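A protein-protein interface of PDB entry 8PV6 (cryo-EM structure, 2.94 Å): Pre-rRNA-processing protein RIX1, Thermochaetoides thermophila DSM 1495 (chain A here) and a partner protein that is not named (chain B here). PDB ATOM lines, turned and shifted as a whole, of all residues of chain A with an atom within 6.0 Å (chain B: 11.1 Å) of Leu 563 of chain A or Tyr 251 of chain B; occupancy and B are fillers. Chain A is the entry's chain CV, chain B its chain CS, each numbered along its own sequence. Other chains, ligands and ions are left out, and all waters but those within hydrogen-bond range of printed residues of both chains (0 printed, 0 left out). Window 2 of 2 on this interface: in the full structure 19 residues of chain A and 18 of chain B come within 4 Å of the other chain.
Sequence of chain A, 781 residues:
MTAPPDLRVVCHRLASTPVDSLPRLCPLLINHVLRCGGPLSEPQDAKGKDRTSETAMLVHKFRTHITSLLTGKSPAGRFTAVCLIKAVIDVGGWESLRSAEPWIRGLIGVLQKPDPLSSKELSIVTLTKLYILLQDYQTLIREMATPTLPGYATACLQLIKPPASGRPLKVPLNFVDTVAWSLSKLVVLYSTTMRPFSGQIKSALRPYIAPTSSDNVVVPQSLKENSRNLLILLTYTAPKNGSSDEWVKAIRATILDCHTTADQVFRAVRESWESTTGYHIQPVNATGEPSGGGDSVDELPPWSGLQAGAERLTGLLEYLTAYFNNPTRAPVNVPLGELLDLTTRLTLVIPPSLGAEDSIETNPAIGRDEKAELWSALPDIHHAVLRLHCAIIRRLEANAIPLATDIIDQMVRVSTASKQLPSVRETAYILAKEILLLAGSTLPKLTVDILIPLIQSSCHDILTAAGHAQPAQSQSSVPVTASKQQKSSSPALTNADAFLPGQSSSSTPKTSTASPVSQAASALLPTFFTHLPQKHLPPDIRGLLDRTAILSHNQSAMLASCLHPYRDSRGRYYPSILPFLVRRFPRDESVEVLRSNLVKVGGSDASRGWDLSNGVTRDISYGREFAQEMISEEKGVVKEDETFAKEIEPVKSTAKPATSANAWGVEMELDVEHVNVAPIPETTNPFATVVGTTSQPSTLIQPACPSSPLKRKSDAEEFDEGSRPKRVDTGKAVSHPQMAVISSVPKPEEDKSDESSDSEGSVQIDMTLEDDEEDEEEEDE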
ATOM      1  N   MET A 558      19.750  25.269   7.897  1.00  0.00           N
ATOM      2  CA  MET A 558      19.599  24.249   6.861  1.00  0.00           C
ATOM      3  C   MET A 558      18.218  24.303   6.218  1.00  0.00           C
ATOM      4  O   MET A 558      18.092  24.174   4.994  1.00  0.00           O
ATOM      5  CB  MET A 558      19.889  22.853   7.416  1.00  0.00           C
ATOM      6  CG  MET A 558      21.278  22.696   8.012  1.00  0.00           C
ATOM      7  SD  MET A 558      21.806  20.981   8.179  1.00  0.00           S
ATOM      8  CE  MET A 558      21.146  20.563   9.783  1.00  0.00           C
ATOM      9  N   LEU A 559      17.166  24.508   7.021  1.00  0.00           N
ATOM     10  CA  LEU A 559      15.840  24.674   6.426  1.00  0.00           C
ATOM     11  C   LEU A 559      15.749  25.934   5.570  1.00  0.00           C
ATOM     12  O   LEU A 559      15.113  25.912   4.507  1.00  0.00           O
ATOM     13  CB  LEU A 559      14.759  24.661   7.511  1.00  0.00           C
ATOM     14  CG  LEU A 559      13.306  24.814   7.050  1.00  0.00           C
ATOM     15  CD1 LEU A 559      12.394  23.944   7.840  1.00  0.00           C
ATOM     16  CD2 LEU A 559      12.859  26.239   7.289  1.00  0.00           C
ATOM     17  N   ALA A 560      16.370  27.031   6.008  1.00  0.00           N
ATOM     18  CA  ALA A 560      16.381  28.249   5.208  1.00  0.00           C
ATOM     19  C   ALA A 560      17.135  28.056   3.902  1.00  0.00           C
ATOM     20  O   ALA A 560      16.713  28.577   2.865  1.00  0.00           O
ATOM     21  CB  ALA A 560      16.992  29.392   6.013  1.00  0.00           C
ATOM     22  N   SER A 561      18.239  27.307   3.929  1.00  0.00           N
ATOM     23  CA  SER A 561      18.970  27.017   2.702  1.00  0.00           C
ATOM     24  C   SER A 561      18.156  26.132   1.768  1.00  0.00           C
ATOM     25  O   SER A 561      18.221  26.291   0.544  1.00  0.00           O
ATOM     26  CB  SER A 561      20.305  26.358   3.029  1.00  0.00           C
ATOM     27  OG  SER A 561      20.942  25.907   1.848  1.00  0.00           O
ATOM     28  N   CYS A 562      17.400  25.182   2.325  1.00  0.00           N
ATOM     29  CA  CYS A 562      16.532  24.352   1.495  1.00  0.00           C
ATOM     30  C   CYS A 562      15.409  25.161   0.858  1.00  0.00           C
ATOM     31  O   CYS A 562      15.067  24.931  -0.306  1.00  0.00           O
ATOM     32  CB  CYS A 562      15.950  23.202   2.315  1.00  0.00           C
ATOM     33  SG  CYS A 562      17.161  21.985   2.855  1.00  0.00           S
ATOM     34  N   LEU A 563      14.827  26.104   1.595  1.00  0.00           N
ATOM     35  CA  LEU A 563      13.689  26.868   1.100  1.00  0.00           C
ATOM     36  C   LEU A 563      14.083  28.115   0.319  1.00  0.00           C
ATOM     37  O   LEU A 563      13.214  28.740  -0.294  1.00  0.00           O
ATOM     38  CB  LEU A 563      12.776  27.256   2.264  1.00  0.00           C
ATOM     39  CG  LEU A 563      12.131  26.066   2.969  1.00  0.00           C
ATOM     40  CD1 LEU A 563      11.177  26.551   4.025  1.00  0.00           C
ATOM     41  CD2 LEU A 563      11.412  25.179   1.967  1.00  0.00           C
ATOM     42  N   HIS A 564      15.360  28.489   0.318  1.00  0.00           N
ATOM     43  CA  HIS A 564      15.859  29.600  -0.492  1.00  0.00           C
ATOM     44  C   HIS A 564      17.026  29.100  -1.330  1.00  0.00           C
ATOM     45  O   HIS A 564      18.195  29.322  -0.995  1.00  0.00           O
ATOM     46  CB  HIS A 564      16.269  30.781   0.389  1.00  0.00           C
ATOM     47  CG  HIS A 564      15.122  31.418   1.106  1.00  0.00           C
ATOM     48  ND1 HIS A 564      14.732  31.038   2.371  1.00  0.00           N
ATOM     49  CD2 HIS A 564      14.275  32.405   0.732  1.00  0.00           C
ATOM     50  CE1 HIS A 564      13.696  31.766   2.747  1.00  0.00           C
ATOM     51  NE2 HIS A 564      13.399  32.604   1.770  1.00  0.00           N
ATOM     52  N   PRO A 565      16.737  28.408  -2.432  1.00  0.00           N
ATOM     53  CA  PRO A 565      17.806  27.765  -3.203  1.00  0.00           C
ATOM     54  C   PRO A 565      18.640  28.774  -3.977  1.00  0.00           C
ATOM     55  O   PRO A 565      18.213  29.900  -4.240  1.00  0.00           O
ATOM     56  CB  PRO A 565      17.045  26.830  -4.146  1.00  0.00           C
ATOM     57  CG  PRO A 565      15.704  27.456  -4.279  1.00  0.00           C
ATOM     58  CD  PRO A 565      15.402  28.111  -2.978  1.00  0.00           C
ATOM     59  N   TYR A 573      18.871  25.163 -10.272  1.00  0.00           N
ATOM     60  CA  TYR A 573      18.971  25.222  -8.824  1.00  0.00           C
ATOM     61  C   TYR A 573      20.054  24.278  -8.309  1.00  0.00           C
ATOM     62  O   TYR A 573      20.284  23.193  -8.849  1.00  0.00           O
ATOM     63  CB  TYR A 573      17.632  24.878  -8.174  1.00  0.00           C
ATOM     64  CG  TYR A 573      16.510  25.830  -8.514  1.00  0.00           C
ATOM     65  CD1 TYR A 573      15.723  25.641  -9.642  1.00  0.00           C
ATOM     66  CD2 TYR A 573      16.242  26.922  -7.706  1.00  0.00           C
ATOM     67  CE1 TYR A 573      14.697  26.514  -9.948  1.00  0.00           C
ATOM     68  CE2 TYR A 573      15.220  27.798  -8.000  1.00  0.00           C
ATOM     69  CZ  TYR A 573      14.450  27.590  -9.123  1.00  0.00           C
ATOM     70  OH  TYR A 573      13.431  28.463  -9.424  1.00  0.00           O
ATOM     71  N   LEU A 594       8.034  20.045   6.186  1.00  0.00           N
ATOM     72  CA  LEU A 594       8.388  19.685   4.820  1.00  0.00           C
ATOM     73  C   LEU A 594       7.771  18.364   4.388  1.00  0.00           C
ATOM     74  O   LEU A 594       7.691  18.099   3.184  1.00  0.00           O
ATOM     75  CB  LEU A 594       9.909  19.626   4.662  1.00  0.00           C
ATOM     76  CG  LEU A 594      10.580  20.981   4.435  1.00  0.00           C
ATOM     77  CD1 LEU A 594      12.087  20.844   4.445  1.00  0.00           C
ATOM     78  CD2 LEU A 594      10.104  21.595   3.129  1.00  0.00           C
ATOM     79  N   PRO B 245      15.072  29.146 -19.733  1.00  0.00           N
ATOM     80  CA  PRO B 245      13.712  29.656 -19.503  1.00  0.00           C
ATOM     81  C   PRO B 245      13.078  29.117 -18.229  1.00  0.00           C
ATOM     82  O   PRO B 245      13.646  28.253 -17.554  1.00  0.00           O
ATOM     83  CB  PRO B 245      12.948  29.190 -20.749  1.00  0.00           C
ATOM     84  CG  PRO B 245      13.715  28.013 -21.239  1.00  0.00           C
ATOM     85  CD  PRO B 245      15.149  28.350 -20.972  1.00  0.00           C
ATOM     86  N   TYR B 246      11.890  29.618 -17.902  1.00  0.00           N
ATOM     87  CA  TYR B 246      11.237  29.321 -16.634  1.00  0.00           C
ATOM     88  C   TYR B 246      10.683  27.902 -16.651  1.00  0.00           C
ATOM     89  O   TYR B 246       9.945  27.527 -17.569  1.00  0.00           O
ATOM     90  CB  TYR B 246      10.119  30.327 -16.365  1.00  0.00           C
ATOM     91  CG  TYR B 246       9.294  30.013 -15.139  1.00  0.00           C
ATOM     92  CD1 TYR B 246       9.864  30.033 -13.873  1.00  0.00           C
ATOM     93  CD2 TYR B 246       7.947  29.695 -15.248  1.00  0.00           C
ATOM     94  CE1 TYR B 246       9.115  29.747 -12.749  1.00  0.00           C
ATOM     95  CE2 TYR B 246       7.191  29.407 -14.130  1.00  0.00           C
ATOM     96  CZ  TYR B 246       7.780  29.433 -12.882  1.00  0.00           C
ATOM     97  OH  TYR B 246       7.032  29.148 -11.765  1.00  0.00           O
ATOM     98  N   LYS B 247      11.042  27.115 -15.636  1.00  0.00           N
ATOM     99  CA  LYS B 247      10.471  25.790 -15.445  1.00  0.00           C
ATOM    100  C   LYS B 247       9.416  25.860 -14.356  1.00  0.00           C
ATOM    101  O   LYS B 247       9.747  26.211 -13.214  1.00  0.00           O
ATOM    102  CB  LYS B 247      11.550  24.781 -15.073  1.00  0.00           C
ATOM    103  CG  LYS B 247      12.677  24.675 -16.083  1.00  0.00           C
ATOM    104  CD  LYS B 247      13.655  23.577 -15.700  1.00  0.00           C
ATOM    105  CE  LYS B 247      14.761  23.437 -16.732  1.00  0.00           C
ATOM    106  NZ  LYS B 247      15.698  22.331 -16.393  1.00  0.00           N
ATOM    107  N   PRO B 248       8.149  25.562 -14.661  1.00  0.00           N
ATOM    108  CA  PRO B 248       7.081  25.731 -13.660  1.00  0.00           C
ATOM    109  C   PRO B 248       7.191  24.812 -12.455  1.00  0.00           C
ATOM    110  O   PRO B 248       6.646  25.151 -11.397  1.00  0.00           O
ATOM    111  CB  PRO B 248       5.803  25.433 -14.458  1.00  0.00           C
ATOM    112  CG  PRO B 248       6.196  25.595 -15.893  1.00  0.00           C
ATOM    113  CD  PRO B 248       7.618  25.149 -15.968  1.00  0.00           C
ATOM    114  N   ARG B 249       7.868  23.671 -12.570  1.00  0.00           N
ATOM    115  CA  ARG B 249       7.948  22.706 -11.482  1.00  0.00           C
ATOM    116  C   ARG B 249       9.409  22.363 -11.184  1.00  0.00           C
ATOM    117  O   ARG B 249       9.799  21.211 -11.035  1.00  0.00           O
ATOM    118  CB  ARG B 249       7.131  21.456 -11.804  1.00  0.00           C
ATOM    119  CG  ARG B 249       7.441  20.804 -13.143  1.00  0.00           C
ATOM    120  CD  ARG B 249       6.789  19.440 -13.215  1.00  0.00           C
ATOM    121  NE  ARG B 249       7.325  18.552 -12.191  1.00  0.00           N
ATOM    122  CZ  ARG B 249       6.711  17.465 -11.746  1.00  0.00           C
ATOM    123  NH1 ARG B 249       5.535  17.091 -12.220  1.00  0.00           N
ATOM    124  NH2 ARG B 249       7.294  16.735 -10.799  1.00  0.00           N
ATOM    125  N   ALA B 250      10.247  23.390 -11.085  1.00  0.00           N
ATOM    126  CA  ALA B 250      11.640  23.197 -10.715  1.00  0.00           C
ATOM    127  C   ALA B 250      11.920  23.428  -9.241  1.00  0.00           C
ATOM    128  O   ALA B 250      12.674  22.645  -8.649  1.00  0.00           O
ATOM    129  CB  ALA B 250      12.550  24.120 -11.539  1.00  0.00           C
ATOM    130  N   TYR B 251      11.323  24.457  -8.631  1.00  0.00           N
ATOM    131  CA  TYR B 251      11.623  24.806  -7.247  1.00  0.00           C
ATOM    132  C   TYR B 251      11.187  23.710  -6.282  1.00  0.00           C
ATOM    133  O   TYR B 251      11.921  23.366  -5.349  1.00  0.00           O
ATOM    134  CB  TYR B 251      10.951  26.133  -6.893  1.00  0.00           C
ATOM    135  CG  TYR B 251      10.853  26.412  -5.412  1.00  0.00           C
ATOM    136  CD1 TYR B 251      11.987  26.686  -4.661  1.00  0.00           C
ATOM    137  CD2 TYR B 251       9.625  26.413  -4.767  1.00  0.00           C
ATOM    138  CE1 TYR B 251      11.901  26.947  -3.309  1.00  0.00           C
ATOM    139  CE2 TYR B 251       9.530  26.674  -3.414  1.00  0.00           C
ATOM    140  CZ  TYR B 251      10.671  26.940  -2.692  1.00  0.00           C
ATOM    141  OH  TYR B 251      10.578  27.199  -1.345  1.00  0.00           O
ATOM    142  N   TRP B 252       9.996  23.149  -6.488  1.00  0.00           N
ATOM    143  CA  TRP B 252       9.519  22.098  -5.600  1.00  0.00           C
ATOM    144  C   TRP B 252      10.135  20.740  -5.904  1.00  0.00           C
ATOM    145  O   TRP B 252      10.337  19.949  -4.975  1.00  0.00           O
ATOM    146  CB  TRP B 252       7.992  22.009  -5.655  1.00  0.00           C
ATOM    147  CG  TRP B 252       7.329  23.050  -4.806  1.00  0.00           C
ATOM    148  CD1 TRP B 252       6.527  24.064  -5.234  1.00  0.00           C
ATOM    149  CD2 TRP B 252       7.426  23.190  -3.381  1.00  0.00           C
ATOM    150  NE1 TRP B 252       6.113  24.824  -4.167  1.00  0.00           N
ATOM    151  CE2 TRP B 252       6.652  24.307  -3.019  1.00  0.00           C
ATOM    152  CE3 TRP B 252       8.089  22.477  -2.378  1.00  0.00           C
ATOM    153  CZ2 TRP B 252       6.525  24.728  -1.699  1.00  0.00           C
ATOM    154  CZ3 TRP B 252       7.961  22.897  -1.069  1.00  0.00           C
ATOM    155  CH2 TRP B 252       7.185  24.011  -0.741  1.00  0.00           C
ATOM    156  N   ASP B 253      10.436  20.450  -7.170  1.00  0.00           N
ATOM    157  CA  ASP B 253      11.138  19.221  -7.510  1.00  0.00           C
ATOM    158  C   ASP B 253      12.571  19.206  -7.007  1.00  0.00           C
ATOM    159  O   ASP B 253      13.088  18.127  -6.698  1.00  0.00           O
ATOM    160  CB  ASP B 253      11.127  18.994  -9.023  1.00  0.00           C
ATOM    161  CG  ASP B 253       9.778  18.531  -9.528  1.00  0.00           C
ATOM    162  OD1 ASP B 253       8.804  18.578  -8.749  1.00  0.00           O
ATOM    163  OD2 ASP B 253       9.689  18.120 -10.703  1.00  0.00           O
ATOM    164  N   ASN B 254      13.209  20.371  -6.887  1.00  0.00           N
ATOM    165  CA  ASN B 254      14.522  20.477  -6.268  1.00  0.00           C
ATOM    166  C   ASN B 254      14.526  20.048  -4.806  1.00  0.00           C
ATOM    167  O   ASN B 254      15.582  19.669  -4.292  1.00  0.00           O
ATOM    168  CB  ASN B 254      15.032  21.917  -6.385  1.00  0.00           C
ATOM    169  CG  ASN B 254      16.510  22.042  -6.080  1.00  0.00           C
ATOM    170  OD1 ASN B 254      17.314  21.206  -6.489  1.00  0.00           O
ATOM    171  ND2 ASN B 254      16.876  23.089  -5.355  1.00  0.00           N
ATOM    172  N   ILE B 255      13.378  20.084  -4.133  1.00  0.00           N
ATOM    173  CA  ILE B 255      13.289  19.706  -2.729  1.00  0.00           C
ATOM    174  C   ILE B 255      12.759  18.283  -2.613  1.00  0.00           C
ATOM    175  O   ILE B 255      13.232  17.500  -1.781  1.00  0.00           O
ATOM    176  CB  ILE B 255      12.400  20.691  -1.948  1.00  0.00           C
ATOM    177  CG1 ILE B 255      12.819  22.132  -2.239  1.00  0.00           C
ATOM    178  CG2 ILE B 255      12.482  20.420  -0.460  1.00  0.00           C
ATOM    179  CD1 ILE B 255      11.972  23.168  -1.534  1.00  0.00           C
ATOM    180  N   TYR B 256      11.785  17.931  -3.448  1.00  0.00           N
ATOM    181  CA  TYR B 256      11.091  16.658  -3.311  1.00  0.00           C
ATOM    182  C   TYR B 256      11.555  15.587  -4.289  1.00  0.00           C
ATOM    183  O   TYR B 256      10.894  14.549  -4.394  1.00  0.00           O
ATOM    184  CB  TYR B 256       9.582  16.864  -3.464  1.00  0.00           C
ATOM    185  CG  TYR B 256       8.949  17.533  -2.270  1.00  0.00           C
ATOM    186  CD1 TYR B 256       9.353  17.216  -0.980  1.00  0.00           C
ATOM    187  CD2 TYR B 256       7.950  18.482  -2.429  1.00  0.00           C
ATOM    188  CE1 TYR B 256       8.782  17.825   0.116  1.00  0.00           C
ATOM    189  CE2 TYR B 256       7.372  19.096  -1.338  1.00  0.00           C
ATOM    190  CZ  TYR B 256       7.793  18.764  -0.069  1.00  0.00           C
ATOM    191  OH  TYR B 256       7.219  19.372   1.023  1.00  0.00           O
ATOM    192  N   ARG B 257      12.656  15.795  -5.008  1.00  0.00           N
ATOM    193  CA  ARG B 257      13.201  14.771  -5.886  1.00  0.00           C
ATOM    194  C   ARG B 257      14.703  14.661  -5.681  1.00  0.00           C
ATOM    195  O   ARG B 257      15.330  15.540  -5.083  1.00  0.00           O
ATOM    196  CB  ARG B 257      12.892  15.059  -7.358  1.00  0.00           C
ATOM    197  CG  ARG B 257      11.417  14.984  -7.705  1.00  0.00           C
ATOM    198  CD  ARG B 257      11.170  15.273  -9.171  1.00  0.00           C
ATOM    199  NE  ARG B 257      11.756  14.250 -10.027  1.00  0.00           N
ATOM    200  CZ  ARG B 257      11.676  14.246 -11.350  1.00  0.00           C
ATOM    201  NH1 ARG B 257      11.033  15.197 -12.005  1.00  0.00           N
ATOM    202  NH2 ARG B 257      12.253  13.260 -12.031  1.00  0.00           N
ATOM    203  N   LEU B 258      15.270  13.561  -6.171  1.00  0.00           N
ATOM    204  CA  LEU B 258      16.696  13.322  -6.033  1.00  0.00           C
ATOM    205  C   LEU B 258      17.491  14.314  -6.883  1.00  0.00           C
ATOM    206  O   LEU B 258      16.998  14.799  -7.905  1.00  0.00           O
ATOM    207  CB  LEU B 258      17.040  11.895  -6.449  1.00  0.00           C
ATOM    208  CG  LEU B 258      16.574  10.764  -5.534  1.00  0.00           C
ATOM    209  CD1 LEU B 258      16.919   9.429  -6.161  1.00  0.00           C
ATOM    210  CD2 LEU B 258      17.203  10.888  -4.161  1.00  0.00           C
ATOM    211  N   PRO B 259      18.713  14.647  -6.470  1.00  0.00           N
ATOM    212  CA  PRO B 259      19.538  15.556  -7.276  1.00  0.00           C
ATOM    213  C   PRO B 259      19.962  14.907  -8.585  1.00  0.00           C
ATOM    214  O   PRO B 259      20.585  13.844  -8.600  1.00  0.00           O
ATOM    215  CB  PRO B 259      20.742  15.836  -6.369  1.00  0.00           C
ATOM    216  CG  PRO B 259      20.254  15.544  -4.991  1.00  0.00           C
ATOM    217  CD  PRO B 259      19.317  14.390  -5.153  1.00  0.00           C
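OH of Tyr 251 of chain B is in hydrogen-bond range of O of Leu 563 of chain A (3.2 Å).
OH of Tyr 256 of chain B is in hydrogen-bond range of O of Leu 594 of chain A.
The backbone carbonyl oxygen (O) of Met 558 of chain A sits at hydrogen-bond distance from the side-chain sulfur (SG) of Cys 562 of chain A (3.2 Å).
Among the printed residues, merely in contact across the chains: Tyr 573 of chain A with Asn 254 of chain B (3.4 Å), Tyr 573 of chain A with Ala 250 of chain B (3.6 Å), Pro 565 of chain A with Tyr 251 of chain B (3.7 Å), Cys 562 of chain A with Ile 255 of chain B (3.8 Å) and Pro 565 of chain A with Asn 254 of chain B (3.9 Å).
No residue of chain B comes within 4 Å of Ala 560 of chain A.
Printed residues of chain B within 4 Å of Leu 563 of chain A: Tyr 251 (3.2 Å).
No residue of chain B comes within 4 Å of His 564 of chain A.
Pro 565 of chain A touches two residues of chain B.
Printed residues of chain B within 4 Å of Leu 594 of chain A: Tyr 256 (2.6 Å).
Of chain A, only Leu 563 (3.2 Å) and Pro 565 (3.7 Å) come within 4 Å of Tyr 251 of chain B.
Of the printed residues of chain A, Ile 255 of chain B touches Cys 562.
Pro 259 of chain B touches none of the printed residues of chain A.
The nearest residue of chain A that does not touch Tyr 251 of chain B is Tyr 573 of chain A (4.2 Å).
The nearest printed residue of chain B that does not touch Leu 594 of chain A is Ile 255 of chain B (4.5 Å).
Hydrophobic or aromatic side chains of chain B within 4 Å of the printed part of chain A: Ala 250, Tyr 251, Ile 255 and Tyr 256.
Of the 10 printed residues of chain A, 5 touch a printed residue of chain B.
Hydrophobic or aromatic side chains of chain A within 4 Å of the printed part of chain B: Leu 563, Pro 565 and Tyr 573.
Among the printed residues, 7 pairs touch across the chains.
Among the printed residues, no Asp or Glu carboxylate lies within 4 Å of a Lys or Arg side-chain nitrogen of the other chain.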
